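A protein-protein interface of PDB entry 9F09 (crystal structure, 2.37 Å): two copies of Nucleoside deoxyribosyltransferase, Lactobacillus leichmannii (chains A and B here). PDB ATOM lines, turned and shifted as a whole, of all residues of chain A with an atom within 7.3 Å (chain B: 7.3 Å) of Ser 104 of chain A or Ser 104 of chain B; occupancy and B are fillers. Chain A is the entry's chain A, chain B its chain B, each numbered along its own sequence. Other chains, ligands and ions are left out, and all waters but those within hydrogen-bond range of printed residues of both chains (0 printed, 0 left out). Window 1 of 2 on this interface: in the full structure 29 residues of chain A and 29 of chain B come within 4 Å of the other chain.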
ATOM      1  N   GLU A  98      26.530  22.917  20.422  1.00  0.00           N
ATOM      2  CA  GLU A  98      27.760  22.357  20.955  1.00  0.00           C
ATOM      3  C   GLU A  98      27.515  21.583  22.246  1.00  0.00           C
ATOM      4  O   GLU A  98      28.174  20.571  22.486  1.00  0.00           O
ATOM      5  CB  GLU A  98      28.737  23.484  21.267  1.00  0.00           C
ATOM      6  CG  GLU A  98      29.303  24.161  20.027  1.00  0.00           C
ATOM      7  CD  GLU A  98      29.953  25.503  20.314  1.00  0.00           C
ATOM      8  OE1 GLU A  98      29.856  26.107  21.429  1.00  0.00           O
ATOM      9  OE2 GLU A  98      30.594  25.916  19.343  1.00  0.00           O
ATOM     10  N   LEU A  99      26.563  22.049  23.069  1.00  0.00           N
ATOM     11  CA  LEU A  99      26.168  21.311  24.268  1.00  0.00           C
ATOM     12  C   LEU A  99      25.638  19.932  23.884  1.00  0.00           C
ATOM     13  O   LEU A  99      26.008  18.921  24.473  1.00  0.00           O
ATOM     14  CB  LEU A  99      25.136  22.088  25.073  1.00  0.00           C
ATOM     15  CG  LEU A  99      25.586  23.434  25.650  1.00  0.00           C
ATOM     16  CD1 LEU A  99      24.427  24.158  26.304  1.00  0.00           C
ATOM     17  CD2 LEU A  99      26.712  23.256  26.659  1.00  0.00           C
ATOM     18  N   GLY A 100      24.784  19.898  22.861  1.00  0.00           N
ATOM     19  CA  GLY A 100      24.215  18.653  22.374  1.00  0.00           C
ATOM     20  C   GLY A 100      25.287  17.737  21.791  1.00  0.00           C
ATOM     21  O   GLY A 100      25.240  16.549  22.012  1.00  0.00           O
ATOM     22  N   TYR A 101      26.285  18.298  21.098  1.00  0.00           N
ATOM     23  CA  TYR A 101      27.353  17.481  20.562  1.00  0.00           C
ATOM     24  C   TYR A 101      28.174  16.916  21.726  1.00  0.00           C
ATOM     25  O   TYR A 101      28.482  15.724  21.737  1.00  0.00           O
ATOM     26  CB  TYR A 101      28.102  18.277  19.490  1.00  0.00           C
ATOM     27  CG  TYR A 101      29.210  17.474  18.831  1.00  0.00           C
ATOM     28  CD1 TYR A 101      28.975  16.540  17.820  1.00  0.00           C
ATOM     29  CD2 TYR A 101      30.511  17.620  19.277  1.00  0.00           C
ATOM     30  CE1 TYR A 101      30.016  15.815  17.244  1.00  0.00           C
ATOM     31  CE2 TYR A 101      31.550  16.882  18.742  1.00  0.00           C
ATOM     32  CZ  TYR A 101      31.310  15.982  17.724  1.00  0.00           C
ATOM     33  OH  TYR A 101      32.427  15.340  17.268  1.00  0.00           O
ATOM     34  N   ALA A 102      28.494  17.765  22.711  1.00  0.00           N
ATOM     35  CA  ALA A 102      29.269  17.343  23.871  1.00  0.00           C
ATOM     36  C   ALA A 102      28.592  16.180  24.589  1.00  0.00           C
ATOM     37  O   ALA A 102      29.251  15.210  24.942  1.00  0.00           O
ATOM     38  CB  ALA A 102      29.466  18.504  24.819  1.00  0.00           C
ATOM     39  N   LEU A 103      27.274  16.280  24.797  1.00  0.00           N
ATOM     40  CA  LEU A 103      26.490  15.206  25.380  1.00  0.00           C
ATOM     41  C   LEU A 103      26.711  13.932  24.576  1.00  0.00           C
ATOM     42  O   LEU A 103      27.015  12.885  25.125  1.00  0.00           O
ATOM     43  CB  LEU A 103      25.005  15.535  25.404  1.00  0.00           C
ATOM     44  CG  LEU A 103      24.078  14.372  25.787  1.00  0.00           C
ATOM     45  CD1 LEU A 103      24.222  14.060  27.275  1.00  0.00           C
ATOM     46  CD2 LEU A 103      22.612  14.639  25.411  1.00  0.00           C
ATOM     47  N   SER A 104      26.589  14.044  23.263  1.00  0.00           N
ATOM     48  CA  SER A 104      26.727  12.878  22.410  1.00  0.00           C
ATOM     49  C   SER A 104      28.139  12.299  22.496  1.00  0.00           C
ATOM     50  O   SER A 104      28.345  11.146  22.140  1.00  0.00           O
ATOM     51  CB  SER A 104      26.394  13.217  20.987  1.00  0.00           C
ATOM     52  OG  SER A 104      27.507  13.795  20.309  1.00  0.00           O
ATOM     53  N   GLN A 105      29.134  13.117  22.877  1.00  0.00           N
ATOM     54  CA  GLN A 105      30.492  12.603  22.909  1.00  0.00           C
ATOM     55  C   GLN A 105      30.880  12.165  24.316  1.00  0.00           C
ATOM     56  O   GLN A 105      32.050  11.878  24.556  1.00  0.00           O
ATOM     57  CB  GLN A 105      31.490  13.651  22.407  1.00  0.00           C
ATOM     58  CG  GLN A 105      31.338  13.979  20.932  1.00  0.00           C
ATOM     59  CD  GLN A 105      31.666  12.800  20.050  1.00  0.00           C
ATOM     60  OE1 GLN A 105      32.687  12.145  20.230  1.00  0.00           O
ATOM     61  NE2 GLN A 105      30.828  12.544  19.065  1.00  0.00           N
ATOM     62  N   GLY A 106      29.917  12.095  25.239  1.00  0.00           N
ATOM     63  CA  GLY A 106      30.172  11.612  26.584  1.00  0.00           C
ATOM     64  C   GLY A 106      30.943  12.581  27.479  1.00  0.00           C
ATOM     65  O   GLY A 106      31.610  12.142  28.403  1.00  0.00           O
ATOM     66  N   LYS A 107      30.846  13.888  27.230  1.00  0.00           N
ATOM     67  CA  LYS A 107      31.606  14.869  27.997  1.00  0.00           C
ATOM     68  C   LYS A 107      30.774  15.388  29.156  1.00  0.00           C
ATOM     69  O   LYS A 107      29.570  15.585  29.019  1.00  0.00           O
ATOM     70  CB  LYS A 107      31.940  16.104  27.146  1.00  0.00           C
ATOM     71  CG  LYS A 107      32.709  15.804  25.859  1.00  0.00           C
ATOM     72  CD  LYS A 107      34.012  15.058  26.109  1.00  0.00           C
ATOM     73  CE  LYS A 107      34.550  14.502  24.816  1.00  0.00           C
ATOM     74  NZ  LYS A 107      35.921  14.019  24.983  1.00  0.00           N
ATOM     75  N   VAL A 109      29.301  18.247  31.021  1.00  0.00           N
ATOM     76  CA  VAL A 109      28.785  19.485  30.475  1.00  0.00           C
ATOM     77  C   VAL A 109      28.504  20.436  31.639  1.00  0.00           C
ATOM     78  O   VAL A 109      27.536  20.257  32.370  1.00  0.00           O
ATOM     79  CB  VAL A 109      27.536  19.280  29.600  1.00  0.00           C
ATOM     80  CG1 VAL A 109      27.048  20.604  29.069  1.00  0.00           C
ATOM     81  CG2 VAL A 109      27.786  18.327  28.449  1.00  0.00           C
ATOM     82  N   VAL A 129      20.498  19.413  29.207  1.00  0.00           N
ATOM     83  CA  VAL A 129      21.744  18.880  28.662  1.00  0.00           C
ATOM     84  C   VAL A 129      22.843  18.940  29.713  1.00  0.00           C
ATOM     85  O   VAL A 129      23.815  18.210  29.624  1.00  0.00           O
ATOM     86  CB  VAL A 129      22.439  19.547  27.469  1.00  0.00           C
ATOM     87  CG1 VAL A 129      22.382  18.746  26.198  1.00  0.00           C
ATOM     88  CG2 VAL A 129      22.142  21.012  27.385  1.00  0.00           C
ATOM     89  N   GLU B  98      18.641  20.675  20.638  1.00  0.00           N
ATOM     90  CA  GLU B  98      17.875  19.584  20.034  1.00  0.00           C
ATOM     91  C   GLU B  98      18.488  19.160  18.696  1.00  0.00           C
ATOM     92  O   GLU B  98      18.449  17.990  18.329  1.00  0.00           O
ATOM     93  CB  GLU B  98      16.437  20.038  19.784  1.00  0.00           C
ATOM     94  CG  GLU B  98      15.614  20.205  21.056  1.00  0.00           C
ATOM     95  CD  GLU B  98      14.313  20.998  20.902  1.00  0.00           C
ATOM     96  OE1 GLU B  98      13.514  20.980  21.870  1.00  0.00           O
ATOM     97  OE2 GLU B  98      14.118  21.697  19.869  1.00  0.00           O
ATOM     98  N   LEU B  99      18.991  20.130  17.927  1.00  0.00           N
ATOM     99  CA  LEU B  99      19.666  19.837  16.671  1.00  0.00           C
ATOM    100  C   LEU B  99      20.885  18.946  16.928  1.00  0.00           C
ATOM    101  O   LEU B  99      21.103  17.954  16.232  1.00  0.00           O
ATOM    102  CB  LEU B  99      20.074  21.144  16.002  1.00  0.00           C
ATOM    103  CG  LEU B  99      18.939  22.056  15.516  1.00  0.00           C
ATOM    104  CD1 LEU B  99      19.530  23.331  14.937  1.00  0.00           C
ATOM    105  CD2 LEU B  99      18.036  21.398  14.466  1.00  0.00           C
ATOM    106  N   GLY B 100      21.671  19.298  17.950  1.00  0.00           N
ATOM    107  CA  GLY B 100      22.820  18.497  18.339  1.00  0.00           C
ATOM    108  C   GLY B 100      22.428  17.085  18.774  1.00  0.00           C
ATOM    109  O   GLY B 100      23.065  16.123  18.388  1.00  0.00           O
ATOM    110  N   TYR B 101      21.328  16.958  19.513  1.00  0.00           N
ATOM    111  CA  TYR B 101      20.856  15.649  19.911  1.00  0.00           C
ATOM    112  C   TYR B 101      20.408  14.861  18.673  1.00  0.00           C
ATOM    113  O   TYR B 101      20.761  13.698  18.534  1.00  0.00           O
ATOM    114  CB  TYR B 101      19.825  15.848  21.032  1.00  0.00           C
ATOM    115  CG  TYR B 101      19.258  14.544  21.561  1.00  0.00           C
ATOM    116  CD1 TYR B 101      19.972  13.753  22.456  1.00  0.00           C
ATOM    117  CD2 TYR B 101      18.049  14.063  21.083  1.00  0.00           C
ATOM    118  CE1 TYR B 101      19.472  12.535  22.895  1.00  0.00           C
ATOM    119  CE2 TYR B 101      17.524  12.871  21.541  1.00  0.00           C
ATOM    120  CZ  TYR B 101      18.235  12.104  22.447  1.00  0.00           C
ATOM    121  OH  TYR B 101      17.666  10.935  22.843  1.00  0.00           O
ATOM    122  N   ALA B 102      19.664  15.493  17.762  1.00  0.00           N
ATOM    123  CA  ALA B 102      19.183  14.835  16.555  1.00  0.00           C
ATOM    124  C   ALA B 102      20.348  14.277  15.733  1.00  0.00           C
ATOM    125  O   ALA B 102      20.292  13.142  15.273  1.00  0.00           O
ATOM    126  CB  ALA B 102      18.370  15.807  15.727  1.00  0.00           C
ATOM    127  N   LEU B 103      21.402  15.080  15.560  1.00  0.00           N
ATOM    128  CA  LEU B 103      22.619  14.639  14.902  1.00  0.00           C
ATOM    129  C   LEU B 103      23.136  13.379  15.583  1.00  0.00           C
ATOM    130  O   LEU B 103      23.406  12.372  14.939  1.00  0.00           O
ATOM    131  CB  LEU B 103      23.694  15.719  14.961  1.00  0.00           C
ATOM    132  CG  LEU B 103      25.092  15.291  14.496  1.00  0.00           C
ATOM    133  CD1 LEU B 103      25.134  14.990  12.979  1.00  0.00           C
ATOM    134  CD2 LEU B 103      26.120  16.350  14.904  1.00  0.00           C
ATOM    135  N   SER B 104      23.223  13.426  16.907  1.00  0.00           N
ATOM    136  CA  SER B 104      23.748  12.300  17.651  1.00  0.00           C
ATOM    137  C   SER B 104      22.859  11.065  17.486  1.00  0.00           C
ATOM    138  O   SER B 104      23.308   9.930  17.699  1.00  0.00           O
ATOM    139  CB  SER B 104      23.894  12.654  19.105  1.00  0.00           C
ATOM    140  OG  SER B 104      22.693  12.452  19.844  1.00  0.00           O
ATOM    141  N   GLN B 105      21.567  11.268  17.186  1.00  0.00           N
ATOM    142  CA  GLN B 105      20.686  10.112  17.075  1.00  0.00           C
ATOM    143  C   GLN B 105      20.585   9.640  15.630  1.00  0.00           C
ATOM    144  O   GLN B 105      19.822   8.743  15.340  1.00  0.00           O
ATOM    145  CB  GLN B 105      19.301  10.407  17.628  1.00  0.00           C
ATOM    146  CG  GLN B 105      19.301  10.643  19.127  1.00  0.00           C
ATOM    147  CD  GLN B 105      19.636   9.398  19.908  1.00  0.00           C
ATOM    148  OE1 GLN B 105      19.161   8.294  19.630  1.00  0.00           O
ATOM    149  NE2 GLN B 105      20.467   9.563  20.914  1.00  0.00           N
ATOM    150  N   GLY B 106      21.383  10.210  14.723  1.00  0.00           N
ATOM    151  CA  GLY B 106      21.417   9.718  13.355  1.00  0.00           C
ATOM    152  C   GLY B 106      20.234  10.196  12.502  1.00  0.00           C
ATOM    153  O   GLY B 106      19.915   9.551  11.521  1.00  0.00           O
ATOM    154  N   LYS B 107      19.597  11.323  12.858  1.00  0.00           N
ATOM    155  CA  LYS B 107      18.435  11.800  12.134  1.00  0.00           C
ATOM    156  C   LYS B 107      18.855  12.774  11.037  1.00  0.00           C
ATOM    157  O   LYS B 107      19.782  13.554  11.223  1.00  0.00           O
ATOM    158  CB  LYS B 107      17.503  12.584  13.066  1.00  0.00           C
ATOM    159  CG  LYS B 107      17.034  11.815  14.298  1.00  0.00           C
ATOM    160  CD  LYS B 107      16.389  10.460  14.008  1.00  0.00           C
ATOM    161  CE  LYS B 107      16.126   9.775  15.287  1.00  0.00           C
ATOM    162  NZ  LYS B 107      15.323   8.564  15.110  1.00  0.00           N
ATOM    163  N   VAL B 109      18.526  16.199   9.540  1.00  0.00           N
ATOM    164  CA  VAL B 109      18.282  17.460  10.213  1.00  0.00           C
ATOM    165  C   VAL B 109      17.971  18.526   9.166  1.00  0.00           C
ATOM    166  O   VAL B 109      18.872  18.999   8.475  1.00  0.00           O
ATOM    167  CB  VAL B 109      19.470  17.891  11.102  1.00  0.00           C
ATOM    168  CG1 VAL B 109      19.159  19.202  11.798  1.00  0.00           C
ATOM    169  CG2 VAL B 109      19.849  16.823  12.131  1.00  0.00           C
ATOM    170  N   VAL B 129      25.310  21.758  11.716  1.00  0.00           N
ATOM    171  CA  VAL B 129      24.544  20.600  12.177  1.00  0.00           C
ATOM    172  C   VAL B 129      23.578  20.166  11.083  1.00  0.00           C
ATOM    173  O   VAL B 129      23.120  19.034  11.113  1.00  0.00           O
ATOM    174  CB  VAL B 129      23.590  20.686  13.385  1.00  0.00           C
ATOM    175  CG1 VAL B 129      24.127  20.021  14.614  1.00  0.00           C
ATOM    176  CG2 VAL B 129      22.999  22.065  13.561  1.00  0.00           C
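CB of Ser 104 of chain A touches CB of Ser 104 of chain B, at 3.2 Å.
The side-chain hydroxyl (OG) of Ser 104 of chain A is in hydrogen-bond range of the backbone carbonyl oxygen (O) of Tyr 101 of chain A (2.6 Å). O of Tyr 101 of chain B sits at hydrogen-bond distance from OG of Ser 104 of chain B, 2.6 Å away.
Ser 104 of chain A touches its own counterpart, Ser 104 of chain B. Positions printed for both chains: 98, 99, 100, 101, 102, 103, 104, 105, 106, 107, 109 and 129.
Printed residues of chain B within 4 Å of Ser 104 of chain A: Ser 104 (3.2 Å). Ser 104 of chain B touches one residue of chain A. Gln 105 of chain A touches none of the printed residues of chain B. The nearest residue of chain B that does not touch Ser 104 of chain A is Gly 100 of chain B (5.1 Å).
Printed residues of chain B that touch a printed residue of chain A: Ser 104. Of the 12 printed residues of chain A, 1 touches a printed residue of chain B. Among the printed residues, no Asp or Glu carboxylate lies within 4 Å of a Lys or Arg side-chain nitrogen of the other chain.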
